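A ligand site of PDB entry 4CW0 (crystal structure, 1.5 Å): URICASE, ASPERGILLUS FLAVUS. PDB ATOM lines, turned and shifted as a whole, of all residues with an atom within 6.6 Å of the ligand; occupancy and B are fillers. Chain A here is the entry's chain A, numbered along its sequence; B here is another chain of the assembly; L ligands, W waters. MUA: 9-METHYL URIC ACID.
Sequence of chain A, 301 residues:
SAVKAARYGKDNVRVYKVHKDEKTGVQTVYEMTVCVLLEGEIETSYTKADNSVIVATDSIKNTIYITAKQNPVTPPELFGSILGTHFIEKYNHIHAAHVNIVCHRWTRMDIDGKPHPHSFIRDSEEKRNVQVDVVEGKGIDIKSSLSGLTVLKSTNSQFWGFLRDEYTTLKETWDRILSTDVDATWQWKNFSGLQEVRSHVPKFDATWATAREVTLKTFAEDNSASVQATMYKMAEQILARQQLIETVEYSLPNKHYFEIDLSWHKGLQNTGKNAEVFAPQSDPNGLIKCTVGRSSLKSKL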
ATOM      1  N   SER A 157     -22.676   1.342 -14.074  1.00  0.00           N
ATOM      2  CA  SER A 157     -23.063   0.103 -14.738  1.00  0.00           C
ATOM      3  C   SER A 157     -24.537  -0.107 -14.378  1.00  0.00           C
ATOM      4  O   SER A 157     -24.943   0.110 -13.225  1.00  0.00           O
ATOM      5  CB  SER A 157     -22.210  -1.077 -14.241  1.00  0.00           C
ATOM      6  OG  SER A 157     -22.704  -2.295 -14.745  1.00  0.00           O
ATOM      7  N   GLN A 158     -25.319  -0.595 -15.347  1.00  0.00           N
ATOM      8  CA  GLN A 158     -26.762  -0.758 -15.254  1.00  0.00           C
ATOM      9  C   GLN A 158     -27.132  -2.080 -15.886  1.00  0.00           C
ATOM     10  O   GLN A 158     -26.404  -2.611 -16.737  1.00  0.00           O
ATOM     11  CB  GLN A 158     -27.520   0.377 -15.958  1.00  0.00           C
ATOM     12  CG  GLN A 158     -27.046   1.754 -15.542  1.00  0.00           C
ATOM     13  CD  GLN A 158     -27.849   2.867 -16.124  1.00  0.00           C
ATOM     14  OE1 GLN A 158     -29.066   2.776 -16.257  1.00  0.00           O
ATOM     15  NE2 GLN A 158     -27.178   3.944 -16.462  1.00  0.00           N
ATOM     16  N   PHE A 159     -28.293  -2.611 -15.494  1.00  0.00           N
ATOM     17  CA  PHE A 159     -28.825  -3.776 -16.210  1.00  0.00           C
ATOM     18  C   PHE A 159     -30.328  -3.860 -15.964  1.00  0.00           C
ATOM     19  O   PHE A 159     -30.797  -4.323 -14.928  1.00  0.00           O
ATOM     20  CB  PHE A 159     -28.103  -5.085 -15.831  1.00  0.00           C
ATOM     21  CG  PHE A 159     -28.414  -6.219 -16.779  1.00  0.00           C
ATOM     22  CD1 PHE A 159     -28.067  -6.137 -18.142  1.00  0.00           C
ATOM     23  CD2 PHE A 159     -29.093  -7.353 -16.341  1.00  0.00           C
ATOM     24  CE1 PHE A 159     -28.409  -7.167 -19.012  1.00  0.00           C
ATOM     25  CE2 PHE A 159     -29.398  -8.403 -17.211  1.00  0.00           C
ATOM     26  CZ  PHE A 159     -29.052  -8.294 -18.533  1.00  0.00           C
ATOM     27  N   PHE A 162     -34.214  -6.377 -19.535  1.00  0.00           N
ATOM     28  CA  PHE A 162     -34.039  -7.754 -19.975  1.00  0.00           C
ATOM     29  C   PHE A 162     -35.362  -8.523 -19.937  1.00  0.00           C
ATOM     30  O   PHE A 162     -36.336  -8.106 -19.305  1.00  0.00           O
ATOM     31  CB  PHE A 162     -32.937  -8.453 -19.167  1.00  0.00           C
ATOM     32  CG  PHE A 162     -33.129  -8.339 -17.677  1.00  0.00           C
ATOM     33  CD1 PHE A 162     -33.892  -9.279 -17.001  1.00  0.00           C
ATOM     34  CD2 PHE A 162     -32.524  -7.297 -16.957  1.00  0.00           C
ATOM     35  CE1 PHE A 162     -34.067  -9.166 -15.633  1.00  0.00           C
ATOM     36  CE2 PHE A 162     -32.707  -7.181 -15.586  1.00  0.00           C
ATOM     37  CZ  PHE A 162     -33.480  -8.123 -14.939  1.00  0.00           C
ATOM     38  N   LEU A 170     -34.438 -11.981 -11.222  1.00  0.00           N
ATOM     39  CA  LEU A 170     -33.481 -10.884 -11.116  1.00  0.00           C
ATOM     40  C   LEU A 170     -34.191  -9.532 -11.111  1.00  0.00           C
ATOM     41  O   LEU A 170     -35.048  -9.238 -11.954  1.00  0.00           O
ATOM     42  CB  LEU A 170     -32.507 -10.919 -12.277  1.00  0.00           C
ATOM     43  CG  LEU A 170     -31.376  -9.908 -12.298  1.00  0.00           C
ATOM     44  CD1 LEU A 170     -30.382 -10.132 -11.156  1.00  0.00           C
ATOM     45  CD2 LEU A 170     -30.683  -9.940 -13.662  1.00  0.00           C
ATOM     46  N   ARG A 176     -25.049  -0.557 -10.420  1.00  0.00           N
ATOM     47  CA  ARG A 176     -24.420  -1.742  -9.871  1.00  0.00           C
ATOM     48  C   ARG A 176     -22.921  -1.637 -10.042  1.00  0.00           C
ATOM     49  O   ARG A 176     -22.401  -0.814 -10.821  1.00  0.00           O
ATOM     50  CB  ARG A 176     -24.950  -3.025 -10.527  1.00  0.00           C
ATOM     51  CG  ARG A 176     -24.542  -3.173 -11.991  1.00  0.00           C
ATOM     52  CD  ARG A 176     -25.009  -4.453 -12.657  1.00  0.00           C
ATOM     53  NE  ARG A 176     -24.495  -4.532 -14.023  1.00  0.00           N
ATOM     54  CZ  ARG A 176     -24.667  -5.558 -14.844  1.00  0.00           C
ATOM     55  NH1 ARG A 176     -25.332  -6.635 -14.488  1.00  0.00           N
ATOM     56  NH2 ARG A 176     -24.106  -5.501 -16.054  1.00  0.00           N
ATOM     57  N   LEU A 178     -19.645  -3.352 -11.596  1.00  0.00           N
ATOM     58  CA  LEU A 178     -19.250  -4.243 -12.663  1.00  0.00           C
ATOM     59  C   LEU A 178     -17.775  -4.601 -12.547  1.00  0.00           C
ATOM     60  O   LEU A 178     -16.920  -3.717 -12.448  1.00  0.00           O
ATOM     61  CB  LEU A 178     -19.548  -3.592 -14.038  1.00  0.00           C
ATOM     62  CG  LEU A 178     -19.137  -4.416 -15.262  1.00  0.00           C
ATOM     63  CD1 LEU A 178     -19.883  -5.762 -15.317  1.00  0.00           C
ATOM     64  CD2 LEU A 178     -19.336  -3.575 -16.512  1.00  0.00           C
ATOM     65  N   SER A 224     -22.541   1.805 -18.553  1.00  0.00           N
ATOM     66  CA  SER A 224     -22.756   0.553 -19.283  1.00  0.00           C
ATOM     67  C   SER A 224     -24.203   0.066 -19.190  1.00  0.00           C
ATOM     68  O   SER A 224     -24.740  -0.079 -18.098  1.00  0.00           O
ATOM     69  CB  SER A 224     -21.856  -0.543 -18.690  1.00  0.00           C
ATOM     70  OG  SER A 224     -22.110  -1.830 -19.226  1.00  0.00           O
ATOM     71  N   ALA A 225     -24.793  -0.278 -20.325  1.00  0.00           N
ATOM     72  CA  ALA A 225     -26.127  -0.831 -20.402  1.00  0.00           C
ATOM     73  C   ALA A 225     -26.159  -2.332 -20.144  1.00  0.00           C
ATOM     74  O   ALA A 225     -27.201  -2.896 -19.832  1.00  0.00           O
ATOM     75  CB  ALA A 225     -26.719  -0.561 -21.773  1.00  0.00           C
ATOM     76  N   SER A 226     -24.988  -2.978 -20.332  1.00  0.00           N
ATOM     77  CA  SER A 226     -24.806  -4.418 -20.190  1.00  0.00           C
ATOM     78  C   SER A 226     -23.338  -4.672 -20.520  1.00  0.00           C
ATOM     79  O   SER A 226     -22.656  -3.838 -21.141  1.00  0.00           O
ATOM     80  CB  SER A 226     -25.669  -5.220 -21.176  1.00  0.00           C
ATOM     81  OG  SER A 226     -25.267  -4.960 -22.505  1.00  0.00           O
ATOM     82  N   VAL A 227     -22.868  -5.846 -20.109  1.00  0.00           N
ATOM     83  CA  VAL A 227     -21.553  -6.296 -20.556  1.00  0.00           C
ATOM     84  C   VAL A 227     -21.496  -6.331 -22.101  1.00  0.00           C
ATOM     85  O   VAL A 227     -20.518  -5.888 -22.712  1.00  0.00           O
ATOM     86  CB  VAL A 227     -21.154  -7.651 -19.942  1.00  0.00           C
ATOM     87  CG1 VAL A 227     -19.794  -8.107 -20.488  1.00  0.00           C
ATOM     88  CG2 VAL A 227     -21.077  -7.520 -18.415  1.00  0.00           C
ATOM     89  N   GLN A 228     -22.540  -6.903 -22.705  1.00  0.00           N
ATOM     90  CA  GLN A 228     -22.678  -7.000 -24.182  1.00  0.00           C
ATOM     91  C   GLN A 228     -22.416  -5.666 -24.865  1.00  0.00           C
ATOM     92  O   GLN A 228     -21.626  -5.580 -25.825  1.00  0.00           O
ATOM     93  CB  GLN A 228     -24.089  -7.481 -24.544  1.00  0.00           C
ATOM     94  CG  GLN A 228     -24.396  -8.941 -24.230  1.00  0.00           C
ATOM     95  CD  GLN A 228     -24.871  -9.238 -22.781  1.00  0.00           C
ATOM     96  OE1 GLN A 228     -24.566  -8.510 -21.828  1.00  0.00           O
ATOM     97  NE2 GLN A 228     -25.542 -10.361 -22.610  1.00  0.00           N
ATOM     98  N   ASN A 254     -19.005 -11.889 -15.905  1.00  0.00           N
ATOM     99  CA  ASN A 254     -19.573 -10.906 -15.028  1.00  0.00           C
ATOM    100  C   ASN A 254     -19.401 -11.421 -13.599  1.00  0.00           C
ATOM    101  O   ASN A 254     -20.062 -12.365 -13.189  1.00  0.00           O
ATOM    102  CB  ASN A 254     -21.051 -10.685 -15.368  1.00  0.00           C
ATOM    103  CG  ASN A 254     -21.636  -9.506 -14.677  1.00  0.00           C
ATOM    104  OD1 ASN A 254     -20.987  -8.878 -13.852  1.00  0.00           O
ATOM    105  ND2 ASN A 254     -22.906  -9.219 -14.973  1.00  0.00           N
ATOM    106  N   HIS A 256     -19.914 -11.207 -10.038  1.00  0.00           N
ATOM    107  CA  HIS A 256     -20.995 -10.496  -9.378  1.00  0.00           C
ATOM    108  C   HIS A 256     -20.589 -10.049  -7.956  1.00  0.00           C
ATOM    109  O   HIS A 256     -19.909 -10.794  -7.229  1.00  0.00           O
ATOM    110  CB  HIS A 256     -22.231 -11.367  -9.310  1.00  0.00           C
ATOM    111  CG  HIS A 256     -22.692 -11.892 -10.656  1.00  0.00           C
ATOM    112  ND1 HIS A 256     -23.171 -11.074 -11.654  1.00  0.00           N
ATOM    113  CD2 HIS A 256     -22.774 -13.152 -11.123  1.00  0.00           C
ATOM    114  CE1 HIS A 256     -23.477 -11.816 -12.701  1.00  0.00           C
ATOM    115  NE2 HIS A 256     -23.258 -13.085 -12.402  1.00  0.00           N
ATOM    116  N   GLY A 286     -21.817 -14.735 -14.791  1.00  0.00           N
ATOM    117  CA  GLY A 286     -22.168 -14.512 -16.186  1.00  0.00           C
ATOM    118  C   GLY A 286     -20.916 -14.719 -17.017  1.00  0.00           C
ATOM    119  O   GLY A 286     -19.797 -14.501 -16.554  1.00  0.00           O
ATOM    120  N   ILE A 288     -19.965 -13.753 -21.066  1.00  0.00           N
ATOM    121  CA  ILE A 288     -20.443 -12.998 -22.209  1.00  0.00           C
ATOM    122  C   ILE A 288     -19.348 -13.012 -23.284  1.00  0.00           C
ATOM    123  O   ILE A 288     -18.211 -12.645 -22.984  1.00  0.00           O
ATOM    124  CB  ILE A 288     -20.808 -11.542 -21.796  1.00  0.00           C
ATOM    125  CG1 ILE A 288     -21.509 -11.467 -20.431  1.00  0.00           C
ATOM    126  CG2 ILE A 288     -21.627 -10.846 -22.886  1.00  0.00           C
ATOM    127  CD1 ILE A 288     -22.858 -12.177 -20.326  1.00  0.00           C
ATOM    128  N   TYR B   8     -23.690 -16.177 -24.917  1.00  0.00           N
ATOM    129  CA  TYR B   8     -23.619 -15.606 -23.540  1.00  0.00           C
ATOM    130  C   TYR B   8     -24.450 -16.535 -22.632  1.00  0.00           C
ATOM    131  O   TYR B   8     -25.357 -17.237 -23.084  1.00  0.00           O
ATOM    132  CB  TYR B   8     -24.144 -14.151 -23.497  1.00  0.00           C
ATOM    133  CG  TYR B   8     -25.634 -14.141 -23.377  1.00  0.00           C
ATOM    134  CD1 TYR B   8     -26.444 -14.484 -24.482  1.00  0.00           C
ATOM    135  CD2 TYR B   8     -26.236 -14.020 -22.164  1.00  0.00           C
ATOM    136  CE1 TYR B   8     -27.814 -14.598 -24.342  1.00  0.00           C
ATOM    137  CE2 TYR B   8     -27.604 -14.111 -22.005  1.00  0.00           C
ATOM    138  CZ  TYR B   8     -28.403 -14.425 -23.104  1.00  0.00           C
ATOM    139  OH  TYR B   8     -29.755 -14.608 -22.976  1.00  0.00           O
ATOM    140  N   GLY B   9     -24.141 -16.534 -21.353  1.00  0.00           N
ATOM    141  CA  GLY B   9     -24.866 -17.308 -20.405  1.00  0.00           C
ATOM    142  C   GLY B   9     -24.239 -17.357 -19.037  1.00  0.00           C
ATOM    143  O   GLY B   9     -23.592 -16.416 -18.641  1.00  0.00           O
ATOM    144  N   LYS B  10     -24.495 -18.450 -18.329  1.00  0.00           N
ATOM    145  CA  LYS B  10     -23.987 -18.603 -16.958  1.00  0.00           C
ATOM    146  C   LYS B  10     -23.019 -19.763 -16.891  1.00  0.00           C
ATOM    147  O   LYS B  10     -23.310 -20.866 -17.383  1.00  0.00           O
ATOM    148  CB  LYS B  10     -25.093 -18.824 -15.928  1.00  0.00           C
ATOM    149  CG  LYS B  10     -24.701 -18.467 -14.497  1.00  0.00           C
ATOM    150  CD  LYS B  10     -24.625 -16.966 -14.326  1.00  0.00           C
ATOM    151  CE  LYS B  10     -25.399 -16.422 -13.177  1.00  0.00           C
ATOM    152  NZ  LYS B  10     -25.309 -14.946 -13.220  1.00  0.00           N
ATOM    153  N   ASN B  51     -31.689  -4.777 -24.371  1.00  0.00           N
ATOM    154  CA  ASN B  51     -31.726  -5.898 -23.459  1.00  0.00           C
ATOM    155  C   ASN B  51     -32.967  -6.784 -23.568  1.00  0.00           C
ATOM    156  O   ASN B  51     -33.008  -7.846 -22.975  1.00  0.00           O
ATOM    157  CB  ASN B  51     -31.492  -5.456 -22.023  1.00  0.00           C
ATOM    158  CG  ASN B  51     -30.054  -5.012 -21.784  1.00  0.00           C
ATOM    159  OD1 ASN B  51     -29.123  -5.459 -22.485  1.00  0.00           O
ATOM    160  ND2 ASN B  51     -29.857  -4.108 -20.827  1.00  0.00           N
ATOM    161  N   ILE B  54     -32.264 -10.360 -24.271  1.00  0.00           N
ATOM    162  CA  ILE B  54     -31.478 -11.117 -23.293  1.00  0.00           C
ATOM    163  C   ILE B  54     -32.333 -11.870 -22.293  1.00  0.00           C
ATOM    164  O   ILE B  54     -33.066 -11.263 -21.498  1.00  0.00           O
ATOM    165  CB  ILE B  54     -30.511 -10.200 -22.548  1.00  0.00           C
ATOM    166  CG1 ILE B  54     -29.495  -9.591 -23.519  1.00  0.00           C
ATOM    167  CG2 ILE B  54     -29.827 -10.980 -21.419  1.00  0.00           C
ATOM    168  CD1 ILE B  54     -28.707 -10.606 -24.286  1.00  0.00           C
ATOM    169  N   VAL B  55     -32.277 -13.191 -22.359  1.00  0.00           N
ATOM    170  CA  VAL B  55     -32.676 -14.074 -21.269  1.00  0.00           C
ATOM    171  C   VAL B  55     -31.580 -13.910 -20.226  1.00  0.00           C
ATOM    172  O   VAL B  55     -30.440 -14.284 -20.472  1.00  0.00           O
ATOM    173  CB  VAL B  55     -32.838 -15.540 -21.719  1.00  0.00           C
ATOM    174  CG1 VAL B  55     -33.221 -16.424 -20.539  1.00  0.00           C
ATOM    175  CG2 VAL B  55     -33.907 -15.653 -22.795  1.00  0.00           C
ATOM    176  N   ALA B  56     -31.886 -13.303 -19.076  1.00  0.00           N
ATOM    177  CA  ALA B  56     -30.816 -12.940 -18.141  1.00  0.00           C
ATOM    178  C   ALA B  56     -30.035 -14.202 -17.764  1.00  0.00           C
ATOM    179  O   ALA B  56     -30.620 -15.291 -17.560  1.00  0.00           O
ATOM    180  CB  ALA B  56     -31.370 -12.282 -16.892  1.00  0.00           C
ATOM    181  N   THR B  57     -28.724 -14.049 -17.603  1.00  0.00           N
ATOM    182  CA  THR B  57     -27.930 -15.186 -17.132  1.00  0.00           C
ATOM    183  C   THR B  57     -28.375 -15.691 -15.764  1.00  0.00           C
ATOM    184  O   THR B  57     -28.342 -16.885 -15.504  1.00  0.00           O
ATOM    185  CB  THR B  57     -26.421 -14.915 -17.158  1.00  0.00           C
ATOM    186  OG1 THR B  57     -26.013 -14.023 -16.112  1.00  0.00           O
ATOM    187  CG2 THR B  57     -25.987 -14.354 -18.515  1.00  0.00           C
ATOM    188  N   ASP B  58     -28.925 -14.783 -14.931  1.00  0.00           N
ATOM    189  CA  ASP B  58     -29.504 -15.225 -13.671  1.00  0.00           C
ATOM    190  C   ASP B  58     -30.693 -16.161 -13.879  1.00  0.00           C
ATOM    191  O   ASP B  58     -30.914 -17.115 -13.096  1.00  0.00           O
ATOM    192  CB  ASP B  58     -29.935 -14.013 -12.832  1.00  0.00           C
ATOM    193  CG  ASP B  58     -30.410 -14.405 -11.462  1.00  0.00           C
ATOM    194  OD1 ASP B  58     -29.531 -14.695 -10.626  1.00  0.00           O
ATOM    195  OD2 ASP B  58     -31.637 -14.416 -11.216  1.00  0.00           O
ATOM    196  N   SER B  59     -31.496 -15.857 -14.909  1.00  0.00           N
ATOM    197  CA  SER B  59     -32.642 -16.703 -15.283  1.00  0.00           C
ATOM    198  C   SER B  59     -32.181 -18.050 -15.850  1.00  0.00           C
ATOM    199  O   SER B  59     -32.786 -19.070 -15.569  1.00  0.00           O
ATOM    200  CB  SER B  59     -33.545 -15.989 -16.273  1.00  0.00           C
ATOM    201  OG  SER B  59     -33.973 -14.722 -15.765  1.00  0.00           O
HETATM  202  N1  MUA L   1     -25.473  -9.132 -19.047  1.00  0.00           N
HETATM  203  C2  MUA L   1     -25.189  -8.257 -17.991  1.00  0.00           C
HETATM  204  O2  MUA L   1     -24.538  -7.234 -18.234  1.00  0.00           O
HETATM  205  N3  MUA L   1     -25.670  -8.528 -16.731  1.00  0.00           N
HETATM  206  C4  MUA L   1     -26.379  -9.625 -16.601  1.00  0.00           C
HETATM  207  C5  MUA L   1     -26.712 -10.568 -17.638  1.00  0.00           C
HETATM  208  C6  MUA L   1     -26.220 -10.291 -18.976  1.00  0.00           C
HETATM  209  O6  MUA L   1     -26.413 -10.985 -19.988  1.00  0.00           O
HETATM  210  N7  MUA L   1     -27.465 -11.619 -17.202  1.00  0.00           N
HETATM  211  C8  MUA L   1     -27.645 -11.389 -15.828  1.00  0.00           C
HETATM  212  N9  MUA L   1     -26.945 -10.143 -15.468  1.00  0.00           N
HETATM  213  C10 MUA L   1     -26.943  -9.539 -14.134  1.00  0.00           C
HETATM  214  O8  MUA L   1     -28.259 -12.052 -14.986  1.00  0.00           O
HETATM  215  O   HOH W   1     -27.454  -6.905 -12.172  1.00  0.00           O
HETATM  216  O   HOH W   2     -24.170 -11.827 -16.374  1.00  0.00           O
HETATM  217  O   HOH W   3     -26.465  -9.121 -10.931  1.00  0.00           O
HETATM  218  O   HOH W   4     -26.705 -12.955 -13.112  1.00  0.00           O
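An oxygen (O8) of the ligand sits at hydrogen-bond distance from the backbone NH of Thr 57 of chain B, 3.3 Å away. OG1 of Thr 57 of chain B lies within hydrogen-bond range of N7 of the ligand, 3.0 Å away. The backbone NH (N) of Asp 58 of chain B lies within hydrogen-bond range of an oxygen (O8) of the ligand, at 2.8 Å. O2 of the ligand is in hydrogen-bond range of NH2 of Arg 176, 2.8 Å away. The side-chain amide nitrogen (NE2) of Gln 228 sits at hydrogen-bond distance from an oxygen (O6) of the ligand (2.8 Å). The backbone NH (N) of Val 227 lies within hydrogen-bond range of an oxygen (O2) of the ligand (2.9 Å). A nitrogen (N3) of the ligand lies close to the side-chain amide nitrogen (ND2) of Asn 254 (3.3 Å).
The side-chain amino group (NZ) of Lys 10 of chain B lies within hydrogen-bond range of the side-chain hydroxyl (OG1) of Thr 57 of chain B, at 3.1 Å. The backbone carbonyl oxygen of Ser 157 is in hydrogen-bond range of the backbone NH of Arg 176 (2.9 Å). N of Gln 228 sits close to OG of Ser 226, at 3.4 Å. A ring nitrogen (NE2) of His 256 is in hydrogen-bond range of the backbone carbonyl oxygen (O) of Asn 254. O of Gly 286 lies within hydrogen-bond range of N of Asn 254, 2.8 Å away. The backbone carbonyl oxygen of Ser 226 is in hydrogen-bond range of the side-chain hydroxyl of Ser 224 (2.8 Å). The side-chain hydroxyl (OH) of Tyr 8 of chain B is in hydrogen-bond range of the backbone carbonyl oxygen (O) of Val 55 of chain B, 2.6 Å away.
Phe 159 touches the ligand (CE2 to C4, 3.3 Å). Leu 170 touches the ligand. Ser 226 touches the ligand (CA to O2, 3.4 Å). CD1 of Ile 288 touches O6 of the ligand, 3.8 Å away. Tyr 8 of chain B touches the ligand (CD2 to O6, 3.7 Å). Ile 54 of chain B touches the ligand. Ala 56 of chain B touches the ligand. Of the 26 residues printed, 13 come within 4 Å of the ligand.
Water W4 lies within hydrogen-bond range of NZ of Lys 10 of chain B, O8 of the ligand, OG1 of Thr 57 of chain B and N of Asp 58 of chain B. Water W2 lies within hydrogen-bond range of the side-chain hydroxyl of Thr 57 of chain B, the side-chain amide nitrogen of Asn 254 and a nitrogen (N7) of the ligand.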
